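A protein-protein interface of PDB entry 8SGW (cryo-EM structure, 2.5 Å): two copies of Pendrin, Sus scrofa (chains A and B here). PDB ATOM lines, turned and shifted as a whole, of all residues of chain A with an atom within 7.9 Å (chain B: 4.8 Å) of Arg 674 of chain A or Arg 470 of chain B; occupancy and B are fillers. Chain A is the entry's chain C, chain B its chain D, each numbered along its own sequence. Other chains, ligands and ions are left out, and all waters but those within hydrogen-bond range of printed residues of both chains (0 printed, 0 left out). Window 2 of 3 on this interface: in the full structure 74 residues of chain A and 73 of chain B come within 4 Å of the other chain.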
ATOM      1  N   ILE A 554     -31.577  13.355  25.620  1.00  0.00           N
ATOM      2  CA  ILE A 554     -32.239  12.114  25.238  1.00  0.00           C
ATOM      3  C   ILE A 554     -32.309  11.208  26.461  1.00  0.00           C
ATOM      4  O   ILE A 554     -31.281  10.784  26.996  1.00  0.00           O
ATOM      5  CB  ILE A 554     -31.520  11.429  24.068  1.00  0.00           C
ATOM      6  CG1 ILE A 554     -31.487  12.356  22.852  1.00  0.00           C
ATOM      7  CG2 ILE A 554     -32.202  10.116  23.721  1.00  0.00           C
ATOM      8  CD1 ILE A 554     -30.677  11.821  21.695  1.00  0.00           C
ATOM      9  N   VAL A 559     -36.545   9.110  24.480  1.00  0.00           N
ATOM     10  CA  VAL A 559     -36.334   7.959  23.600  1.00  0.00           C
ATOM     11  C   VAL A 559     -37.555   7.714  22.729  1.00  0.00           C
ATOM     12  O   VAL A 559     -37.458   7.642  21.495  1.00  0.00           O
ATOM     13  CB  VAL A 559     -35.978   6.703  24.416  1.00  0.00           C
ATOM     14  CG1 VAL A 559     -35.901   5.514  23.509  1.00  0.00           C
ATOM     15  CG2 VAL A 559     -34.621   6.871  25.063  1.00  0.00           C
ATOM     16  N   LYS A 563     -37.819   8.487  18.671  1.00  0.00           N
ATOM     17  CA  LYS A 563     -38.169   7.447  17.709  1.00  0.00           C
ATOM     18  C   LYS A 563     -39.348   7.877  16.847  1.00  0.00           C
ATOM     19  O   LYS A 563     -39.313   7.738  15.615  1.00  0.00           O
ATOM     20  CB  LYS A 563     -38.475   6.135  18.432  1.00  0.00           C
ATOM     21  CG  LYS A 563     -37.268   5.500  19.099  1.00  0.00           C
ATOM     22  CD  LYS A 563     -37.633   4.190  19.774  1.00  0.00           C
ATOM     23  CE  LYS A 563     -36.426   3.569  20.459  1.00  0.00           C
ATOM     24  NZ  LYS A 563     -36.768   2.288  21.137  1.00  0.00           N
ATOM     25  N   LEU A 668     -27.489  12.440  28.768  1.00  0.00           N
ATOM     26  CA  LEU A 668     -27.820  11.201  28.085  1.00  0.00           C
ATOM     27  C   LEU A 668     -27.671  10.052  29.071  1.00  0.00           C
ATOM     28  O   LEU A 668     -26.687   9.989  29.811  1.00  0.00           O
ATOM     29  CB  LEU A 668     -26.919  11.003  26.862  1.00  0.00           C
ATOM     30  CG  LEU A 668     -27.143   9.811  25.941  1.00  0.00           C
ATOM     31  CD1 LEU A 668     -28.510   9.888  25.303  1.00  0.00           C
ATOM     32  CD2 LEU A 668     -26.072   9.812  24.878  1.00  0.00           C
ATOM     33  N   ASP A 669     -28.652   9.155  29.082  1.00  0.00           N
ATOM     34  CA  ASP A 669     -28.688   8.032  30.008  1.00  0.00           C
ATOM     35  C   ASP A 669     -28.505   6.723  29.244  1.00  0.00           C
ATOM     36  O   ASP A 669     -28.360   6.703  28.020  1.00  0.00           O
ATOM     37  CB  ASP A 669     -29.996   8.033  30.802  1.00  0.00           C
ATOM     38  CG  ASP A 669     -31.219   8.081  29.911  1.00  0.00           C
ATOM     39  OD1 ASP A 669     -31.061   8.341  28.702  1.00  0.00           O
ATOM     40  OD2 ASP A 669     -32.336   7.860  30.421  1.00  0.00           O
ATOM     41  N   VAL A 670     -28.515   5.614  29.990  1.00  0.00           N
ATOM     42  CA  VAL A 670     -28.291   4.306  29.380  1.00  0.00           C
ATOM     43  C   VAL A 670     -29.414   3.968  28.407  1.00  0.00           C
ATOM     44  O   VAL A 670     -29.179   3.366  27.353  1.00  0.00           O
ATOM     45  CB  VAL A 670     -28.129   3.221  30.464  1.00  0.00           C
ATOM     46  CG1 VAL A 670     -26.874   3.476  31.278  1.00  0.00           C
ATOM     47  CG2 VAL A 670     -29.348   3.166  31.369  1.00  0.00           C
ATOM     48  N   VAL A 671     -30.650   4.346  28.743  1.00  0.00           N
ATOM     49  CA  VAL A 671     -31.770   4.108  27.838  1.00  0.00           C
ATOM     50  C   VAL A 671     -31.582   4.893  26.547  1.00  0.00           C
ATOM     51  O   VAL A 671     -31.841   4.385  25.448  1.00  0.00           O
ATOM     52  CB  VAL A 671     -33.100   4.456  28.532  1.00  0.00           C
ATOM     53  CG1 VAL A 671     -34.276   4.160  27.615  1.00  0.00           C
ATOM     54  CG2 VAL A 671     -33.231   3.690  29.836  1.00  0.00           C
ATOM     55  N   GLY A 672     -31.119   6.139  26.656  1.00  0.00           N
ATOM     56  CA  GLY A 672     -30.855   6.928  25.464  1.00  0.00           C
ATOM     57  C   GLY A 672     -29.747   6.347  24.607  1.00  0.00           C
ATOM     58  O   GLY A 672     -29.836   6.350  23.378  1.00  0.00           O
ATOM     59  N   VAL A 673     -28.686   5.846  25.241  1.00  0.00           N
ATOM     60  CA  VAL A 673     -27.592   5.232  24.492  1.00  0.00           C
ATOM     61  C   VAL A 673     -28.071   3.971  23.782  1.00  0.00           C
ATOM     62  O   VAL A 673     -27.727   3.722  22.617  1.00  0.00           O
ATOM     63  CB  VAL A 673     -26.402   4.947  25.426  1.00  0.00           C
ATOM     64  CG1 VAL A 673     -25.297   4.221  24.678  1.00  0.00           C
ATOM     65  CG2 VAL A 673     -25.880   6.241  26.023  1.00  0.00           C
ATOM     66  N   ARG A 674     -28.870   3.153  24.474  1.00  0.00           N
ATOM     67  CA  ARG A 674     -29.444   1.971  23.840  1.00  0.00           C
ATOM     68  C   ARG A 674     -30.316   2.360  22.658  1.00  0.00           C
ATOM     69  O   ARG A 674     -30.269   1.717  21.604  1.00  0.00           O
ATOM     70  CB  ARG A 674     -30.263   1.168  24.850  1.00  0.00           C
ATOM     71  CG  ARG A 674     -29.463   0.520  25.960  1.00  0.00           C
ATOM     72  CD  ARG A 674     -30.394  -0.010  27.036  1.00  0.00           C
ATOM     73  NE  ARG A 674     -29.710  -0.254  28.299  1.00  0.00           N
ATOM     74  CZ  ARG A 674     -30.322  -0.332  29.472  1.00  0.00           C
ATOM     75  NH1 ARG A 674     -31.633  -0.191  29.577  1.00  0.00           N
ATOM     76  NH2 ARG A 674     -29.603  -0.556  30.567  1.00  0.00           N
ATOM     77  N   SER A 675     -31.120   3.413  22.816  1.00  0.00           N
ATOM     78  CA  SER A 675     -31.967   3.877  21.723  1.00  0.00           C
ATOM     79  C   SER A 675     -31.141   4.340  20.535  1.00  0.00           C
ATOM     80  O   SER A 675     -31.498   4.074  19.384  1.00  0.00           O
ATOM     81  CB  SER A 675     -32.860   5.012  22.204  1.00  0.00           C
ATOM     82  OG  SER A 675     -33.704   5.467  21.161  1.00  0.00           O
ATOM     83  N   LEU A 676     -30.049   5.059  20.794  1.00  0.00           N
ATOM     84  CA  LEU A 676     -29.199   5.520  19.703  1.00  0.00           C
ATOM     85  C   LEU A 676     -28.568   4.346  18.966  1.00  0.00           C
ATOM     86  O   LEU A 676     -28.534   4.329  17.729  1.00  0.00           O
ATOM     87  CB  LEU A 676     -28.128   6.469  20.238  1.00  0.00           C
ATOM     88  CG  LEU A 676     -28.650   7.810  20.757  1.00  0.00           C
ATOM     89  CD1 LEU A 676     -27.511   8.671  21.270  1.00  0.00           C
ATOM     90  CD2 LEU A 676     -29.437   8.539  19.679  1.00  0.00           C
ATOM     91  N   ARG A 677     -28.078   3.346  19.705  1.00  0.00           N
ATOM     92  CA  ARG A 677     -27.522   2.165  19.049  1.00  0.00           C
ATOM     93  C   ARG A 677     -28.583   1.441  18.229  1.00  0.00           C
ATOM     94  O   ARG A 677     -28.320   1.005  17.103  1.00  0.00           O
ATOM     95  CB  ARG A 677     -26.895   1.211  20.068  1.00  0.00           C
ATOM     96  CG  ARG A 677     -25.666   1.758  20.758  1.00  0.00           C
ATOM     97  CD  ARG A 677     -25.090   0.780  21.769  1.00  0.00           C
ATOM     98  NE  ARG A 677     -25.958   0.564  22.920  1.00  0.00           N
ATOM     99  CZ  ARG A 677     -25.731  -0.343  23.859  1.00  0.00           C
ATOM    100  NH1 ARG A 677     -24.674  -1.138  23.810  1.00  0.00           N
ATOM    101  NH2 ARG A 677     -26.583  -0.455  24.873  1.00  0.00           N
ATOM    102  N   MET A 678     -29.791   1.301  18.781  1.00  0.00           N
ATOM    103  CA  MET A 678     -30.857   0.631  18.046  1.00  0.00           C
ATOM    104  C   MET A 678     -31.217   1.391  16.777  1.00  0.00           C
ATOM    105  O   MET A 678     -31.412   0.783  15.722  1.00  0.00           O
ATOM    106  CB  MET A 678     -32.089   0.453  18.932  1.00  0.00           C
ATOM    107  CG  MET A 678     -31.875  -0.475  20.114  1.00  0.00           C
ATOM    108  SD  MET A 678     -31.513  -2.168  19.609  1.00  0.00           S
ATOM    109  CE  MET A 678     -31.092  -2.907  21.184  1.00  0.00           C
ATOM    110  N   ILE A 679     -31.308   2.719  16.859  1.00  0.00           N
ATOM    111  CA  ILE A 679     -31.629   3.517  15.680  1.00  0.00           C
ATOM    112  C   ILE A 679     -30.550   3.355  14.618  1.00  0.00           C
ATOM    113  O   ILE A 679     -30.847   3.148  13.432  1.00  0.00           O
ATOM    114  CB  ILE A 679     -31.822   4.994  16.075  1.00  0.00           C
ATOM    115  CG1 ILE A 679     -33.202   5.206  16.698  1.00  0.00           C
ATOM    116  CG2 ILE A 679     -31.635   5.906  14.872  1.00  0.00           C
ATOM    117  CD1 ILE A 679     -34.348   4.872  15.769  1.00  0.00           C
ATOM    118  N   VAL A 680     -29.281   3.428  15.029  1.00  0.00           N
ATOM    119  CA  VAL A 680     -28.184   3.294  14.076  1.00  0.00           C
ATOM    120  C   VAL A 680     -28.219   1.925  13.408  1.00  0.00           C
ATOM    121  O   VAL A 680     -28.086   1.817  12.184  1.00  0.00           O
ATOM    122  CB  VAL A 680     -26.835   3.552  14.771  1.00  0.00           C
ATOM    123  CG1 VAL A 680     -25.687   3.173  13.853  1.00  0.00           C
ATOM    124  CG2 VAL A 680     -26.724   5.008  15.179  1.00  0.00           C
ATOM    125  N   LYS A 681     -28.413   0.863  14.193  1.00  0.00           N
ATOM    126  CA  LYS A 681     -28.434  -0.483  13.625  1.00  0.00           C
ATOM    127  C   LYS A 681     -29.625  -0.675  12.692  1.00  0.00           C
ATOM    128  O   LYS A 681     -29.487  -1.245  11.602  1.00  0.00           O
ATOM    129  CB  LYS A 681     -28.449  -1.525  14.741  1.00  0.00           C
ATOM    130  CG  LYS A 681     -27.197  -1.530  15.605  1.00  0.00           C
ATOM    131  CD  LYS A 681     -25.944  -1.732  14.772  1.00  0.00           C
ATOM    132  CE  LYS A 681     -24.698  -1.723  15.644  1.00  0.00           C
ATOM    133  NZ  LYS A 681     -23.459  -1.933  14.847  1.00  0.00           N
ATOM    134  N   LEU A 703     -21.439   8.551  25.944  1.00  0.00           N
ATOM    135  CA  LEU A 703     -21.608   7.502  24.945  1.00  0.00           C
ATOM    136  C   LEU A 703     -20.498   6.463  25.046  1.00  0.00           C
ATOM    137  O   LEU A 703     -20.759   5.255  25.051  1.00  0.00           O
ATOM    138  CB  LEU A 703     -21.636   8.113  23.544  1.00  0.00           C
ATOM    139  CG  LEU A 703     -22.959   8.697  23.053  1.00  0.00           C
ATOM    140  CD1 LEU A 703     -22.779   9.333  21.688  1.00  0.00           C
ATOM    141  CD2 LEU A 703     -24.022   7.619  23.001  1.00  0.00           C
ATOM    142  N   GLN A 705     -18.473   5.717  27.540  1.00  0.00           N
ATOM    143  CA  GLN A 705     -18.479   4.918  28.759  1.00  0.00           C
ATOM    144  C   GLN A 705     -19.740   4.074  28.900  1.00  0.00           C
ATOM    145  O   GLN A 705     -19.772   3.174  29.745  1.00  0.00           O
ATOM    146  CB  GLN A 705     -18.309   5.797  30.000  1.00  0.00           C
ATOM    147  CG  GLN A 705     -19.468   6.718  30.308  1.00  0.00           C
ATOM    148  CD  GLN A 705     -19.207   7.559  31.540  1.00  0.00           C
ATOM    149  OE1 GLN A 705     -18.169   7.424  32.187  1.00  0.00           O
ATOM    150  NE2 GLN A 705     -20.151   8.426  31.877  1.00  0.00           N
ATOM    151  N   CYS A 706     -20.771   4.337  28.100  1.00  0.00           N
ATOM    152  CA  CYS A 706     -21.960   3.496  28.066  1.00  0.00           C
ATOM    153  C   CYS A 706     -21.866   2.389  27.024  1.00  0.00           C
ATOM    154  O   CYS A 706     -22.872   1.727  26.749  1.00  0.00           O
ATOM    155  CB  CYS A 706     -23.208   4.345  27.808  1.00  0.00           C
ATOM    156  SG  CYS A 706     -23.762   5.318  29.224  1.00  0.00           S
ATOM    157  N   PHE A 708     -21.309   2.656  23.754  1.00  0.00           N
ATOM    158  CA  PHE A 708     -21.860   2.983  22.443  1.00  0.00           C
ATOM    159  C   PHE A 708     -20.906   2.591  21.321  1.00  0.00           C
ATOM    160  O   PHE A 708     -21.332   2.034  20.304  1.00  0.00           O
ATOM    161  CB  PHE A 708     -22.184   4.474  22.370  1.00  0.00           C
ATOM    162  CG  PHE A 708     -22.855   4.890  21.094  1.00  0.00           C
ATOM    163  CD1 PHE A 708     -24.227   4.802  20.959  1.00  0.00           C
ATOM    164  CD2 PHE A 708     -22.114   5.378  20.032  1.00  0.00           C
ATOM    165  CE1 PHE A 708     -24.846   5.184  19.790  1.00  0.00           C
ATOM    166  CE2 PHE A 708     -22.730   5.760  18.861  1.00  0.00           C
ATOM    167  CZ  PHE A 708     -24.097   5.664  18.740  1.00  0.00           C
ATOM    168  N   ASP B 217     -36.208   1.978  32.538  1.00  0.00           N
ATOM    169  CA  ASP B 217     -35.617   0.651  32.687  1.00  0.00           C
ATOM    170  C   ASP B 217     -34.877   0.462  34.007  1.00  0.00           C
ATOM    171  O   ASP B 217     -35.020  -0.619  34.604  1.00  0.00           O
ATOM    172  CB  ASP B 217     -34.694   0.357  31.497  1.00  0.00           C
ATOM    173  CG  ASP B 217     -35.444  -0.204  30.306  1.00  0.00           C
ATOM    174  OD1 ASP B 217     -36.449  -0.912  30.518  1.00  0.00           O
ATOM    175  OD2 ASP B 217     -35.027   0.064  29.159  1.00  0.00           O
ATOM    176  N   CYS B 466     -27.220  -8.713  39.140  1.00  0.00           N
ATOM    177  CA  CYS B 466     -26.010  -8.889  38.346  1.00  0.00           C
ATOM    178  C   CYS B 466     -25.775  -7.705  37.416  1.00  0.00           C
ATOM    179  O   CYS B 466     -24.625  -7.322  37.173  1.00  0.00           O
ATOM    180  CB  CYS B 466     -26.094 -10.188  37.546  1.00  0.00           C
ATOM    181  SG  CYS B 466     -25.829 -11.680  38.524  1.00  0.00           S
ATOM    182  N   ASP B 467     -26.844  -7.121  36.870  1.00  0.00           N
ATOM    183  CA  ASP B 467     -26.674  -6.006  35.947  1.00  0.00           C
ATOM    184  C   ASP B 467     -26.630  -4.656  36.651  1.00  0.00           C
ATOM    185  O   ASP B 467     -26.404  -3.637  35.989  1.00  0.00           O
ATOM    186  CB  ASP B 467     -27.772  -6.034  34.870  1.00  0.00           C
ATOM    187  CG  ASP B 467     -29.172  -5.760  35.414  1.00  0.00           C
ATOM    188  OD1 ASP B 467     -30.120  -6.395  34.910  1.00  0.00           O
ATOM    189  OD2 ASP B 467     -29.351  -4.892  36.293  1.00  0.00           O
ATOM    190  N   VAL B 468     -26.869  -4.619  37.963  1.00  0.00           N
ATOM    191  CA  VAL B 468     -26.681  -3.368  38.709  1.00  0.00           C
ATOM    192  C   VAL B 468     -25.256  -2.825  38.607  1.00  0.00           C
ATOM    193  O   VAL B 468     -25.097  -1.622  38.342  1.00  0.00           O
ATOM    194  CB  VAL B 468     -27.132  -3.547  40.170  1.00  0.00           C
ATOM    195  CG1 VAL B 468     -26.856  -2.281  40.965  1.00  0.00           C
ATOM    196  CG2 VAL B 468     -28.594  -3.879  40.226  1.00  0.00           C
ATOM    197  N   PRO B 469     -24.192  -3.615  38.832  1.00  0.00           N
ATOM    198  CA  PRO B 469     -22.839  -3.024  38.783  1.00  0.00           C
ATOM    199  C   PRO B 469     -22.446  -2.454  37.427  1.00  0.00           C
ATOM    200  O   PRO B 469     -21.775  -1.415  37.373  1.00  0.00           O
ATOM    201  CB  PRO B 469     -21.934  -4.195  39.192  1.00  0.00           C
ATOM    202  CG  PRO B 469     -22.819  -5.112  39.946  1.00  0.00           C
ATOM    203  CD  PRO B 469     -24.139  -5.024  39.262  1.00  0.00           C
ATOM    204  N   ARG B 470     -22.832  -3.101  36.326  1.00  0.00           N
ATOM    205  CA  ARG B 470     -22.533  -2.525  35.018  1.00  0.00           C
ATOM    206  C   ARG B 470     -23.329  -1.247  34.797  1.00  0.00           C
ATOM    207  O   ARG B 470     -22.859  -0.323  34.125  1.00  0.00           O
ATOM    208  CB  ARG B 470     -22.785  -3.552  33.907  1.00  0.00           C
ATOM    209  CG  ARG B 470     -24.200  -4.110  33.803  1.00  0.00           C
ATOM    210  CD  ARG B 470     -25.102  -3.257  32.920  1.00  0.00           C
ATOM    211  NE  ARG B 470     -26.403  -3.879  32.706  1.00  0.00           N
ATOM    212  CZ  ARG B 470     -27.417  -3.295  32.084  1.00  0.00           C
ATOM    213  NH1 ARG B 470     -27.309  -2.077  31.579  1.00  0.00           N
ATOM    214  NH2 ARG B 470     -28.568  -3.951  31.962  1.00  0.00           N
ATOM    215  N   LEU B 471     -24.536  -1.174  35.364  1.00  0.00           N
ATOM    216  CA  LEU B 471     -25.289   0.075  35.347  1.00  0.00           C
ATOM    217  C   LEU B 471     -24.545   1.172  36.095  1.00  0.00           C
ATOM    218  O   LEU B 471     -24.494   2.319  35.639  1.00  0.00           O
ATOM    219  CB  LEU B 471     -26.675  -0.144  35.953  1.00  0.00           C
ATOM    220  CG  LEU B 471     -27.827   0.710  35.428  1.00  0.00           C
ATOM    221  CD1 LEU B 471     -28.020   0.506  33.936  1.00  0.00           C
ATOM    222  CD2 LEU B 471     -29.101   0.388  36.187  1.00  0.00           C
ATOM    223  N   TRP B 472     -23.960   0.838  37.247  1.00  0.00           N
ATOM    224  CA  TRP B 472     -23.181   1.822  37.993  1.00  0.00           C
ATOM    225  C   TRP B 472     -21.971   2.285  37.194  1.00  0.00           C
ATOM    226  O   TRP B 472     -21.649   3.478  37.175  1.00  0.00           O
ATOM    227  CB  TRP B 472     -22.746   1.238  39.338  1.00  0.00           C
ATOM    228  CG  TRP B 472     -21.806   2.113  40.112  1.00  0.00           C
ATOM    229  CD1 TRP B 472     -20.446   2.023  40.144  1.00  0.00           C
ATOM    230  CD2 TRP B 472     -22.156   3.199  40.979  1.00  0.00           C
ATOM    231  NE1 TRP B 472     -19.926   2.989  40.969  1.00  0.00           N
ATOM    232  CE2 TRP B 472     -20.956   3.724  41.495  1.00  0.00           C
ATOM    233  CE3 TRP B 472     -23.367   3.780  41.366  1.00  0.00           C
ATOM    234  CZ2 TRP B 472     -20.931   4.801  42.376  1.00  0.00           C
ATOM    235  CZ3 TRP B 472     -23.339   4.850  42.241  1.00  0.00           C
ATOM    236  CH2 TRP B 472     -22.129   5.349  42.737  1.00  0.00           C
ATOM    237  N   ARG B 473     -21.287   1.352  36.532  1.00  0.00           N
ATOM    238  CA  ARG B 473     -20.135   1.726  35.715  1.00  0.00           C
ATOM    239  C   ARG B 473     -20.538   2.585  34.523  1.00  0.00           C
ATOM    240  O   ARG B 473     -19.788   3.484  34.129  1.00  0.00           O
ATOM    241  CB  ARG B 473     -19.395   0.478  35.238  1.00  0.00           C
ATOM    242  CG  ARG B 473     -18.311   0.001  36.188  1.00  0.00           C
ATOM    243  CD  ARG B 473     -17.480  -1.107  35.561  1.00  0.00           C
ATOM    244  NE  ARG B 473     -18.306  -2.229  35.133  1.00  0.00           N
ATOM    245  CZ  ARG B 473     -18.737  -3.192  35.936  1.00  0.00           C
ATOM    246  NH1 ARG B 473     -18.438  -3.203  37.225  1.00  0.00           N
ATOM    247  NH2 ARG B 473     -19.488  -4.167  35.434  1.00  0.00           N
ATOM    248  N   GLN B 474     -21.709   2.329  33.938  1.00  0.00           N
ATOM    249  CA  GLN B 474     -22.120   3.044  32.736  1.00  0.00           C
ATOM    250  C   GLN B 474     -22.669   4.430  33.060  1.00  0.00           C
ATOM    251  O   GLN B 474     -22.301   5.416  32.414  1.00  0.00           O
ATOM    252  CB  GLN B 474     -23.164   2.223  31.976  1.00  0.00           C
ATOM    253  CG  GLN B 474     -22.592   1.037  31.224  1.00  0.00           C
ATOM    254  CD  GLN B 474     -23.655   0.255  30.483  1.00  0.00           C
ATOM    255  OE1 GLN B 474     -24.833   0.300  30.834  1.00  0.00           O
ATOM    256  NE2 GLN B 474     -23.243  -0.473  29.452  1.00  0.00           N
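No position is printed for both chains.
Of the 7 pairs that touch across the chains among the printed residues, none has its exchanged pair printed and touching as well.
The guanidinium group of Arg 470 of chain B sits close to the guanidinium group of Arg 674 of chain A, 2.9 Å away.
The backbone carbonyl oxygen (O) of Gln 474 of chain B lies within hydrogen-bond range of the side-chain sulfur (SG) of Cys 706 of chain A (3.5 Å).
The guanidinium group (NH1) of Arg 674 of chain A lies within salt-bridge range of the side-chain carboxylate (OD2) of Asp 217 of chain B (3.4 Å).
Of the 21 printed residues of chain A, 4 touch a printed residue of chain B.
Hydrophobic or aromatic side chains of chain A within 4 Å of the printed part of chain B: Val 670.
Hydrophobic or aromatic side chains of chain B within 4 Å of the printed part of chain A: Leu 471.
Lys 563 of chain A touches none of the printed residues of chain B.
Of the printed residues of chain B, Val 670 of chain A touches Leu 471 and Gln 474.
Val 671 of chain A touches none of the printed residues of chain B.
Arg 470 of chain B touches one residue of chain A.
Printed residues of chain A within 4 Å of Leu 471 of chain B: Val 670 (3.9 Å) and Arg 674 (3.9 Å).
Of the printed residues of chain A, Gln 474 of chain B touches Val 670 (3.8 Å), Gln 705 (3.7 Å) and Cys 706 (3.5 Å).
The nearest printed residue of chain B that does not touch Val 670 of chain A is Arg 470 of chain B (5.5 Å).
CG2 of Val 670 of chain A touches CD1 of Leu 471 of chain B, 3.9 Å away.
Val 670 of chain A touches Gln 474 of chain B.
Arg 674 of chain A touches Leu 471 of chain B (NH2 to CD1, 3.9 Å).
NE2 of Gln 705 of chain A touches O of Gln 474 of chain B (3.7 Å).
O of Asp 467 of chain B lies close to NE of Arg 470 of chain B, 3.3 Å away.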
